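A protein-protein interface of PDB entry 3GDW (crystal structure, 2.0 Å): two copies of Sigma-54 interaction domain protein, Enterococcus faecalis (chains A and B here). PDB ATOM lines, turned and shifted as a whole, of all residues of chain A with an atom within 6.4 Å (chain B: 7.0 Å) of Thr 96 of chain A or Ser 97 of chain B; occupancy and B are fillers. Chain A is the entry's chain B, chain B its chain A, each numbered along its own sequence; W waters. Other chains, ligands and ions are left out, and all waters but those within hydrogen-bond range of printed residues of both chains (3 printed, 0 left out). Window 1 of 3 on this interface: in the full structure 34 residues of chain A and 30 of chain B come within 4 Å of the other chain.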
ATOM      1  N   VAL A   9       4.163  -0.528  -4.738  1.00  0.00           N
ATOM      2  CA  VAL A   9       4.330  -1.467  -3.618  1.00  0.00           C
ATOM      3  C   VAL A   9       4.892  -0.692  -2.424  1.00  0.00           C
ATOM      4  O   VAL A   9       6.006  -0.173  -2.502  1.00  0.00           O
ATOM      5  CB  VAL A   9       5.302  -2.671  -3.981  1.00  0.00           C
ATOM      6  CG1 VAL A   9       5.338  -3.668  -2.857  1.00  0.00           C
ATOM      7  CG2 VAL A   9       4.896  -3.366  -5.301  1.00  0.00           C
ATOM      8  N   MET A  11       5.695  -0.846   1.742  1.00  0.00           N
ATOM      9  CA  MET A  11       5.823  -1.754   2.908  1.00  0.00           C
ATOM     10  C   MET A  11       6.723  -1.217   4.014  1.00  0.00           C
ATOM     11  O   MET A  11       7.601  -0.387   3.772  1.00  0.00           O
ATOM     12  CB  MET A  11       6.312  -3.159   2.463  1.00  0.00           C
ATOM     13  CG  MET A  11       5.324  -3.863   1.569  1.00  0.00           C
ATOM     14  SD  MET A  11       5.964  -5.523   0.873  1.00  0.00           S
ATOM     15  CE  MET A  11       4.384  -5.950  -0.177  1.00  0.00           C
ATOM     16  N   MET A  20      10.878  -7.503  -3.085  1.00  0.00           N
ATOM     17  CA  MET A  20       9.767  -8.240  -3.692  1.00  0.00           C
ATOM     18  C   MET A  20       9.507  -7.806  -5.117  1.00  0.00           C
ATOM     19  O   MET A  20       9.262  -8.665  -5.973  1.00  0.00           O
ATOM     20  CB  MET A  20       8.457  -8.064  -2.929  1.00  0.00           C
ATOM     21  CG  MET A  20       8.275  -8.941  -1.793  1.00  0.00           C
ATOM     22  SD  MET A  20       6.469  -8.650  -1.095  1.00  0.00           S
ATOM     23  CE  MET A  20       6.770  -9.692   0.500  1.00  0.00           C
ATOM     24  N   LEU A  68      -2.395  -0.017  -5.234  1.00  0.00           N
ATOM     25  CA  LEU A  68      -1.465   0.022  -4.084  1.00  0.00           C
ATOM     26  C   LEU A  68      -1.444  -1.335  -3.418  1.00  0.00           C
ATOM     27  O   LEU A  68      -2.493  -1.841  -2.991  1.00  0.00           O
ATOM     28  CB  LEU A  68      -1.914   1.043  -3.028  1.00  0.00           C
ATOM     29  CG  LEU A  68      -2.059   2.504  -3.472  1.00  0.00           C
ATOM     30  CD1 LEU A  68      -2.251   3.409  -2.245  1.00  0.00           C
ATOM     31  CD2 LEU A  68      -0.843   3.002  -4.297  1.00  0.00           C
ATOM     32  N   LEU A  69      -0.260  -1.911  -3.346  1.00  0.00           N
ATOM     33  CA  LEU A  69      -0.033  -3.171  -2.659  1.00  0.00           C
ATOM     34  C   LEU A  69       0.755  -2.860  -1.395  1.00  0.00           C
ATOM     35  O   LEU A  69       1.881  -2.372  -1.468  1.00  0.00           O
ATOM     36  CB  LEU A  69       0.785  -4.086  -3.589  1.00  0.00           C
ATOM     37  CG  LEU A  69       0.101  -4.488  -4.899  1.00  0.00           C
ATOM     38  CD1 LEU A  69       1.033  -5.396  -5.703  1.00  0.00           C
ATOM     39  CD2 LEU A  69      -1.268  -5.189  -4.640  1.00  0.00           C
ATOM     40  N   THR A  70       0.163  -3.111  -0.233  1.00  0.00           N
ATOM     41  CA  THR A  70       0.809  -2.806   1.037  1.00  0.00           C
ATOM     42  C   THR A  70       0.930  -4.063   1.925  1.00  0.00           C
ATOM     43  O   THR A  70       0.411  -5.133   1.594  1.00  0.00           O
ATOM     44  CB  THR A  70       0.010  -1.706   1.825  1.00  0.00           C
ATOM     45  OG1 THR A  70      -1.262  -2.242   2.267  1.00  0.00           O
ATOM     46  CG2 THR A  70      -0.213  -0.460   0.946  1.00  0.00           C
ATOM     47  N   ASP A  71       1.601  -3.918   3.060  1.00  0.00           N
ATOM     48  CA  ASP A  71       1.701  -5.010   4.006  1.00  0.00           C
ATOM     49  C   ASP A  71       0.681  -4.882   5.155  1.00  0.00           C
ATOM     50  O   ASP A  71      -0.147  -5.780   5.340  1.00  0.00           O
ATOM     51  CB  ASP A  71       3.154  -5.226   4.508  1.00  0.00           C
ATOM     52  CG  ASP A  71       3.833  -3.933   5.021  1.00  0.00           C
ATOM     53  OD1 ASP A  71       3.208  -2.819   5.041  1.00  0.00           O
ATOM     54  OD2 ASP A  71       5.009  -4.045   5.432  1.00  0.00           O
ATOM     55  N   MET A  72       0.749  -3.807   5.936  1.00  0.00           N
ATOM     56  CA  MET A  72      -0.046  -3.700   7.163  1.00  0.00           C
ATOM     57  C   MET A  72      -0.158  -2.235   7.601  1.00  0.00           C
ATOM     58  O   MET A  72       0.313  -1.336   6.900  1.00  0.00           O
ATOM     59  CB  MET A  72       0.608  -4.534   8.267  1.00  0.00           C
ATOM     60  CG  MET A  72       2.060  -4.132   8.499  1.00  0.00           C
ATOM     61  SD  MET A  72       2.920  -5.039   9.908  1.00  0.00           S
ATOM     62  CE  MET A  72       1.642  -4.642  11.348  1.00  0.00           C
ATOM     63  N   ILE A  93      -4.568  -3.108  -1.627  1.00  0.00           N
ATOM     64  CA  ILE A  93      -4.612  -4.479  -1.129  1.00  0.00           C
ATOM     65  C   ILE A  93      -3.528  -4.655  -0.069  1.00  0.00           C
ATOM     66  O   ILE A  93      -2.353  -4.403  -0.350  1.00  0.00           O
ATOM     67  CB  ILE A  93      -4.408  -5.482  -2.305  1.00  0.00           C
ATOM     68  CG1 ILE A  93      -5.647  -5.452  -3.212  1.00  0.00           C
ATOM     69  CG2 ILE A  93      -4.110  -6.906  -1.795  1.00  0.00           C
ATOM     70  CD1 ILE A  93      -5.503  -6.213  -4.513  1.00  0.00           C
ATOM     71  N   THR A  94      -3.940  -5.079   1.132  1.00  0.00           N
ATOM     72  CA  THR A  94      -3.036  -5.389   2.250  1.00  0.00           C
ATOM     73  C   THR A  94      -2.509  -6.827   2.195  1.00  0.00           C
ATOM     74  O   THR A  94      -2.960  -7.628   1.375  1.00  0.00           O
ATOM     75  CB  THR A  94      -3.736  -5.223   3.635  1.00  0.00           C
ATOM     76  OG1 THR A  94      -4.832  -6.137   3.746  1.00  0.00           O
ATOM     77  CG2 THR A  94      -4.246  -3.830   3.830  1.00  0.00           C
ATOM     78  N   MET A  95      -1.566  -7.135   3.094  1.00  0.00           N
ATOM     79  CA  MET A  95      -1.054  -8.501   3.293  1.00  0.00           C
ATOM     80  C   MET A  95      -0.362  -8.998   2.021  1.00  0.00           C
ATOM     81  O   MET A  95      -0.371 -10.178   1.720  1.00  0.00           O
ATOM     82  CB  MET A  95      -2.178  -9.464   3.758  1.00  0.00           C
ATOM     83  CG  MET A  95      -2.918  -9.030   5.016  1.00  0.00           C
ATOM     84  SD  MET A  95      -1.788  -9.024   6.630  1.00  0.00           S
ATOM     85  CE  MET A  95      -2.304  -7.255   7.317  1.00  0.00           C
ATOM     86  N   THR A  96       0.206  -8.063   1.264  1.00  0.00           N
ATOM     87  CA  THR A  96       0.821  -8.390  -0.020  1.00  0.00           C
ATOM     88  C   THR A  96       2.066  -9.254   0.194  1.00  0.00           C
ATOM     89  O   THR A  96       2.840  -9.007   1.098  1.00  0.00           O
ATOM     90  CB  THR A  96       1.205  -7.126  -0.795  1.00  0.00           C
ATOM     91  OG1 THR A  96       0.038  -6.326  -1.014  1.00  0.00           O
ATOM     92  CG2 THR A  96       1.768  -7.498  -2.148  1.00  0.00           C
ATOM     93  N   SER A  97       2.205 -10.309  -0.613  1.00  0.00           N
ATOM     94  CA  SER A  97       3.381 -11.163  -0.601  1.00  0.00           C
ATOM     95  C   SER A  97       3.961 -11.197  -2.032  1.00  0.00           C
ATOM     96  O   SER A  97       3.384 -10.636  -2.939  1.00  0.00           O
ATOM     97  CB  SER A  97       2.992 -12.575  -0.136  1.00  0.00           C
ATOM     98  OG  SER A  97       4.154 -13.326   0.178  1.00  0.00           O
ATOM     99  N   THR A  98       5.101 -11.861  -2.211  1.00  0.00           N
ATOM    100  CA  THR A  98       5.821 -11.903  -3.506  1.00  0.00           C
ATOM    101  C   THR A  98       4.910 -12.290  -4.671  1.00  0.00           C
ATOM    102  O   THR A  98       4.931 -11.650  -5.710  1.00  0.00           O
ATOM    103  CB  THR A  98       7.001 -12.904  -3.414  1.00  0.00           C
ATOM    104  OG1 THR A  98       7.664 -12.715  -2.163  1.00  0.00           O
ATOM    105  CG2 THR A  98       8.009 -12.663  -4.532  1.00  0.00           C
ATOM    106  N   ILE A 100       1.708 -12.059  -5.044  1.00  0.00           N
ATOM    107  CA  ILE A 100       0.728 -11.011  -5.307  1.00  0.00           C
ATOM    108  C   ILE A 100       1.383  -9.884  -6.113  1.00  0.00           C
ATOM    109  O   ILE A 100       0.791  -9.431  -7.086  1.00  0.00           O
ATOM    110  CB  ILE A 100       0.117 -10.432  -3.998  1.00  0.00           C
ATOM    111  CG1 ILE A 100      -0.593 -11.522  -3.190  1.00  0.00           C
ATOM    112  CG2 ILE A 100      -0.884  -9.348  -4.327  1.00  0.00           C
ATOM    113  CD1 ILE A 100      -1.553 -12.363  -4.041  1.00  0.00           C
ATOM    114  N   VAL A 101       2.589  -9.449  -5.730  1.00  0.00           N
ATOM    115  CA  VAL A 101       3.331  -8.467  -6.552  1.00  0.00           C
ATOM    116  C   VAL A 101       3.518  -9.045  -7.979  1.00  0.00           C
ATOM    117  O   VAL A 101       3.232  -8.378  -8.989  1.00  0.00           O
ATOM    118  CB  VAL A 101       4.708  -8.076  -5.941  1.00  0.00           C
ATOM    119  CG1 VAL A 101       5.421  -7.039  -6.818  1.00  0.00           C
ATOM    120  CG2 VAL A 101       4.554  -7.558  -4.497  1.00  0.00           C
ATOM    121  N   PHE A 125      -5.799 -14.815  -2.828  1.00  0.00           N
ATOM    122  CA  PHE A 125      -5.928 -14.793  -1.387  1.00  0.00           C
ATOM    123  C   PHE A 125      -6.886 -15.906  -0.941  1.00  0.00           C
ATOM    124  O   PHE A 125      -6.542 -16.674  -0.041  1.00  0.00           O
ATOM    125  CB  PHE A 125      -6.372 -13.419  -0.876  1.00  0.00           C
ATOM    126  CG  PHE A 125      -5.227 -12.453  -0.652  1.00  0.00           C
ATOM    127  CD1 PHE A 125      -4.450 -12.515   0.505  1.00  0.00           C
ATOM    128  CD2 PHE A 125      -4.919 -11.505  -1.593  1.00  0.00           C
ATOM    129  CE1 PHE A 125      -3.387 -11.623   0.713  1.00  0.00           C
ATOM    130  CE2 PHE A 125      -3.871 -10.606  -1.392  1.00  0.00           C
ATOM    131  CZ  PHE A 125      -3.106 -10.668  -0.235  1.00  0.00           C
ATOM    132  N   MET B  11      12.192 -16.551   1.755  1.00  0.00           N
ATOM    133  CA  MET B  11      11.544 -15.719   0.714  1.00  0.00           C
ATOM    134  C   MET B  11      12.427 -15.616  -0.528  1.00  0.00           C
ATOM    135  O   MET B  11      13.660 -15.636  -0.432  1.00  0.00           O
ATOM    136  CB  MET B  11      11.292 -14.295   1.212  1.00  0.00           C
ATOM    137  CG  MET B  11      10.475 -14.168   2.499  1.00  0.00           C
ATOM    138  SD  MET B  11       8.645 -14.811   2.273  1.00  0.00           S
ATOM    139  CE  MET B  11       7.890 -13.188   1.545  1.00  0.00           C
ATOM    140  N   MET B  20      12.071  -8.296   6.239  1.00  0.00           N
ATOM    141  CA  MET B  20      10.870  -8.507   7.035  1.00  0.00           C
ATOM    142  C   MET B  20      11.256  -8.910   8.450  1.00  0.00           C
ATOM    143  O   MET B  20      10.672  -8.405   9.413  1.00  0.00           O
ATOM    144  CB  MET B  20       9.927  -9.563   6.435  1.00  0.00           C
ATOM    145  CG  MET B  20       9.220  -9.170   5.151  1.00  0.00           C
ATOM    146  SD  MET B  20       7.926 -10.564   4.725  1.00  0.00           S
ATOM    147  CE  MET B  20       9.188 -11.988   4.663  1.00  0.00           C
ATOM    148  N   LEU B  69       7.956 -19.735   7.368  1.00  0.00           N
ATOM    149  CA  LEU B  69       7.195 -18.660   6.776  1.00  0.00           C
ATOM    150  C   LEU B  69       7.776 -18.443   5.372  1.00  0.00           C
ATOM    151  O   LEU B  69       8.901 -17.989   5.221  1.00  0.00           O
ATOM    152  CB  LEU B  69       7.307 -17.377   7.645  1.00  0.00           C
ATOM    153  CG  LEU B  69       6.864 -17.509   9.113  1.00  0.00           C
ATOM    154  CD1 LEU B  69       6.959 -16.138   9.838  1.00  0.00           C
ATOM    155  CD2 LEU B  69       5.420 -18.118   9.263  1.00  0.00           C
ATOM    156  N   THR B  70       6.984 -18.734   4.343  1.00  0.00           N
ATOM    157  CA  THR B  70       7.506 -18.806   2.992  1.00  0.00           C
ATOM    158  C   THR B  70       6.631 -17.987   2.058  1.00  0.00           C
ATOM    159  O   THR B  70       5.549 -17.542   2.426  1.00  0.00           O
ATOM    160  CB  THR B  70       7.522 -20.269   2.438  1.00  0.00           C
ATOM    161  OG1 THR B  70       6.180 -20.747   2.318  1.00  0.00           O
ATOM    162  CG2 THR B  70       8.327 -21.219   3.302  1.00  0.00           C
ATOM    163  N   ILE B  93       3.527 -21.686   6.731  1.00  0.00           N
ATOM    164  CA  ILE B  93       2.581 -20.661   6.302  1.00  0.00           C
ATOM    165  C   ILE B  93       3.141 -20.043   5.026  1.00  0.00           C
ATOM    166  O   ILE B  93       4.293 -19.593   4.999  1.00  0.00           O
ATOM    167  CB  ILE B  93       2.357 -19.600   7.414  1.00  0.00           C
ATOM    168  CG1 ILE B  93       1.645 -20.247   8.606  1.00  0.00           C
ATOM    169  CG2 ILE B  93       1.530 -18.410   6.905  1.00  0.00           C
ATOM    170  CD1 ILE B  93       1.600 -19.429   9.823  1.00  0.00           C
ATOM    171  N   THR B  94       2.319 -20.029   3.983  1.00  0.00           N
ATOM    172  CA  THR B  94       2.693 -19.458   2.696  1.00  0.00           C
ATOM    173  C   THR B  94       2.180 -18.033   2.607  1.00  0.00           C
ATOM    174  O   THR B  94       1.535 -17.537   3.546  1.00  0.00           O
ATOM    175  CB  THR B  94       2.131 -20.284   1.515  1.00  0.00           C
ATOM    176  OG1 THR B  94       0.711 -20.109   1.428  1.00  0.00           O
ATOM    177  CG2 THR B  94       2.443 -21.735   1.703  1.00  0.00           C
ATOM    178  N   MET B  95       2.478 -17.379   1.486  1.00  0.00           N
ATOM    179  CA  MET B  95       2.077 -15.998   1.232  1.00  0.00           C
ATOM    180  C   MET B  95       2.425 -15.105   2.426  1.00  0.00           C
ATOM    181  O   MET B  95       1.643 -14.300   2.875  1.00  0.00           O
ATOM    182  CB  MET B  95       0.601 -15.893   0.795  1.00  0.00           C
ATOM    183  CG  MET B  95       0.424 -14.869  -0.354  1.00  0.00           C
ATOM    184  SD  MET B  95      -1.415 -14.741  -0.804  1.00  0.00           S
ATOM    185  CE  MET B  95      -1.322 -15.880  -2.402  1.00  0.00           C
ATOM    186  N   THR B  96       3.626 -15.307   2.945  1.00  0.00           N
ATOM    187  CA  THR B  96       4.109 -14.573   4.090  1.00  0.00           C
ATOM    188  C   THR B  96       4.252 -13.088   3.761  1.00  0.00           C
ATOM    189  O   THR B  96       4.737 -12.734   2.685  1.00  0.00           O
ATOM    190  CB  THR B  96       5.426 -15.194   4.580  1.00  0.00           C
ATOM    191  OG1 THR B  96       5.123 -16.482   5.141  1.00  0.00           O
ATOM    192  CG2 THR B  96       6.068 -14.319   5.643  1.00  0.00           C
ATOM    193  N   SER B  97       3.751 -12.233   4.653  1.00  0.00           N
ATOM    194  CA  SER B  97       3.978 -10.780   4.574  1.00  0.00           C
ATOM    195  C   SER B  97       4.470 -10.285   5.916  1.00  0.00           C
ATOM    196  O   SER B  97       4.520 -11.047   6.873  1.00  0.00           O
ATOM    197  CB  SER B  97       2.678 -10.056   4.207  1.00  0.00           C
ATOM    198  OG  SER B  97       1.648 -10.381   5.130  1.00  0.00           O
ATOM    199  N   THR B  98       4.819  -8.997   5.986  1.00  0.00           N
ATOM    200  CA  THR B  98       5.379  -8.399   7.195  1.00  0.00           C
ATOM    201  C   THR B  98       4.600  -8.739   8.490  1.00  0.00           C
ATOM    202  O   THR B  98       5.201  -9.149   9.491  1.00  0.00           O
ATOM    203  CB  THR B  98       5.506  -6.869   7.029  1.00  0.00           C
ATOM    204  OG1 THR B  98       6.156  -6.588   5.779  1.00  0.00           O
ATOM    205  CG2 THR B  98       6.337  -6.265   8.165  1.00  0.00           C
ATOM    206  N   MET B  99       3.284  -8.572   8.463  1.00  0.00           N
ATOM    207  CA  MET B  99       2.495  -8.831   9.661  1.00  0.00           C
ATOM    208  C   MET B  99       2.515 -10.300  10.094  1.00  0.00           C
ATOM    209  O   MET B  99       2.389 -10.589  11.286  1.00  0.00           O
ATOM    210  CB  MET B  99       1.063  -8.346   9.492  1.00  0.00           C
ATOM    211  CG  MET B  99       0.136  -8.989  10.482  1.00  0.00           C
ATOM    212  SD  MET B  99      -1.598  -8.145  10.528  1.00  0.00           S
ATOM    213  CE  MET B  99      -2.669  -9.770  10.631  1.00  0.00           C
ATOM    214  N   ILE B 100       2.675 -11.216   9.135  1.00  0.00           N
ATOM    215  CA  ILE B 100       2.831 -12.650   9.446  1.00  0.00           C
ATOM    216  C   ILE B 100       4.136 -12.876  10.243  1.00  0.00           C
ATOM    217  O   ILE B 100       4.132 -13.492  11.322  1.00  0.00           O
ATOM    218  CB  ILE B 100       2.817 -13.597   8.180  1.00  0.00           C
ATOM    219  CG1 ILE B 100       1.507 -13.480   7.360  1.00  0.00           C
ATOM    220  CG2 ILE B 100       3.081 -15.057   8.592  1.00  0.00           C
ATOM    221  CD1 ILE B 100       0.269 -13.503   8.178  1.00  0.00           C
ATOM    222  N   VAL B 101       5.241 -12.339   9.725  1.00  0.00           N
ATOM    223  CA  VAL B 101       6.515 -12.439  10.421  1.00  0.00           C
ATOM    224  C   VAL B 101       6.421 -11.760  11.793  1.00  0.00           C
ATOM    225  O   VAL B 101       6.859 -12.322  12.792  1.00  0.00           O
ATOM    226  CB  VAL B 101       7.676 -11.858   9.575  1.00  0.00           C
ATOM    227  CG1 VAL B 101       9.005 -12.005  10.336  1.00  0.00           C
ATOM    228  CG2 VAL B 101       7.753 -12.583   8.194  1.00  0.00           C
ATOM    229  N   LEU B 102       5.847 -10.563  11.839  1.00  0.00           N
ATOM    230  CA  LEU B 102       5.725  -9.812  13.098  1.00  0.00           C
ATOM    231  C   LEU B 102       5.042 -10.649  14.193  1.00  0.00           C
ATOM    232  O   LEU B 102       5.627 -10.878  15.257  1.00  0.00           O
ATOM    233  CB  LEU B 102       4.978  -8.492  12.868  1.00  0.00           C
ATOM    234  CG  LEU B 102       4.831  -7.505  14.033  1.00  0.00           C
ATOM    235  CD1 LEU B 102       6.181  -7.098  14.586  1.00  0.00           C
ATOM    236  CD2 LEU B 102       4.049  -6.282  13.567  1.00  0.00           C
ATOM    237  N   PHE B 125      -4.916 -14.077   9.458  1.00  0.00           N
ATOM    238  CA  PHE B 125      -4.784 -13.953   8.022  1.00  0.00           C
ATOM    239  C   PHE B 125      -6.181 -14.000   7.385  1.00  0.00           C
ATOM    240  O   PHE B 125      -6.521 -13.171   6.544  1.00  0.00           O
ATOM    241  CB  PHE B 125      -3.884 -15.042   7.472  1.00  0.00           C
ATOM    242  CG  PHE B 125      -3.704 -14.990   5.990  1.00  0.00           C
ATOM    243  CD1 PHE B 125      -2.818 -14.084   5.404  1.00  0.00           C
ATOM    244  CD2 PHE B 125      -4.419 -15.854   5.169  1.00  0.00           C
ATOM    245  CE1 PHE B 125      -2.656 -14.053   4.005  1.00  0.00           C
ATOM    246  CE2 PHE B 125      -4.292 -15.829   3.785  1.00  0.00           C
ATOM    247  CZ  PHE B 125      -3.398 -14.943   3.195  1.00  0.00           C
HETATM  248  O   HOH W   1       1.638  -7.873   6.252  1.00  0.00           O
HETATM  249  O   HOH W   2       4.851  -8.004   2.976  1.00  0.00           O
HETATM  250  O   HOH W   3       0.083 -12.106   3.881  1.00  0.00           O
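Among the printed residues, pairs that only touch across the chains: Thr 96 of chain A with Ser 97 of chain B (3.3 Å), Ser 97 of chain A with Met 95 of chain B (3.3 Å), Met 95 of chain A with Met 99 of chain B (3.4 Å), Met 72 of chain A with Leu 102 of chain B (3.7 Å), Thr 98 of chain A with Met 11 of chain B (3.7 Å), Met 95 of chain A with Ser 97 of chain B (3.8 Å), Phe 125 of chain A with Phe 125 of chain B (3.8 Å), Met 72 of chain A with Met 99 of chain B (3.8 Å), Met 20 of chain A with Met 11 of chain B (3.8 Å), Ile 100 of chain A with Met 95 of chain B (3.9 Å), Ser 97 of chain A with Met 11 of chain B (3.98 Å) and Phe 125 of chain A with Met 95 of chain B (3.98 Å).
The side-chain hydroxyl (OG1) of Thr 98 of chain B is in hydrogen-bond range of the side-chain carboxylate (OD2) of Asp 71 of chain A, 2.8 Å away. OG of Ser 97 of chain A sits at hydrogen-bond distance from O of Thr 96 of chain B (2.6 Å).
Printed residues of chain B that touch a printed residue of chain A: Met 11, Met 95, Thr 96, Ser 97, Thr 98, Met 99, Leu 102 and Phe 125. Along chain B the printed residues that touch a printed residue of chain A span positions 11 to 125. Of the 17 printed residues of chain A, 9 touch a printed residue of chain B. Hydrophobic or aromatic side chains of chain A that line the printed part of chain B: Met 20, Met 72, Met 95, Ile 100 and Phe 125. Among the printed residues, 14 pairs touch across the chains.
Printed residues of chain B within 4 Å of Thr 96 of chain A: Ser 97. Of the printed residues of chain B, Ser 97 of chain A touches Met 11 (3.98 Å), Met 95 (3.3 Å) and Thr 96 (2.6 Å). Of the printed residues of chain A, Met 11 of chain B touches Met 20, Ser 97 and Thr 98. Of the printed residues of chain A, Ser 97 of chain B touches Met 95 (3.8 Å) and Thr 96 (3.3 Å). The nearest residue of chain B that does not touch Thr 96 of chain A is Thr 96 of chain B (4.5 Å). The nearest residue of chain A that does not touch Ser 97 of chain B is Ser 97 of chain A (4.6 Å).
Water W3 lies within hydrogen-bond range of the side-chain hydroxyl (OG) of Ser 97 of chain B (2.6 Å), the backbone carbonyl oxygen (O) of Met 95 of chain B (2.9 Å) and the backbone carbonyl oxygen (O) of Met 95 of chain A (2.9 Å). Water W1 lies within hydrogen-bond range of OG of Ser 97 of chain B (2.7 Å), N of Met 99 of chain B (2.8 Å), O of Asp 71 of chain A (2.9 Å), N of Thr 98 of chain B (3.4 Å) and SD of Met 95 of chain A (3.6 Å). Water W2 lies within hydrogen-bond range of the backbone carbonyl oxygen of Thr 96 of chain A, the backbone NH of Thr 98 of chain B and the side-chain sulfur of Met 11 of chain A.
Met 20 of chain A touches Met 11 of chain B, but with the chains exchanged Met 11 of chain A does not touch Met 20 of chain B (6.5 Å). Met 95 of chain A touches Ser 97 of chain B, and with the chains exchanged Ser 97 of chain A touches Met 95 of chain B. Phe 125 of chain A touches Met 95 of chain B, but with the chains exchanged Met 95 of chain A does not touch Phe 125 of chain B (4.6 Å). Phe 125 of chain A touches its own counterpart, Phe 125 of chain B. Of the 14 pairs that touch across the chains among the printed residues, 5 have their exchanged pair printed and touching as well.
OG1 of Thr 96 of chain B sits at hydrogen-bond distance from O of Thr 70 of chain B, at 2.9 Å. The backbone NH (N) of Met 95 of chain A sits at hydrogen-bond distance from the backbone carbonyl oxygen (O) of Thr 70 of chain A. SD of Met 20 of chain A lies within hydrogen-bond range of N of Thr 98 of chain A, 3.7 Å away. N of Thr 98 of chain B lies within hydrogen-bond range of SD of Met 20 of chain B, at 3.7 Å. The backbone NH (N) of Met 95 of chain A sits at hydrogen-bond distance from the backbone carbonyl oxygen (O) of Asp 71 of chain A, at 3.0 Å. O of Thr 70 of chain B lies within hydrogen-bond range of N of Met 95 of chain B (3.2 Å).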
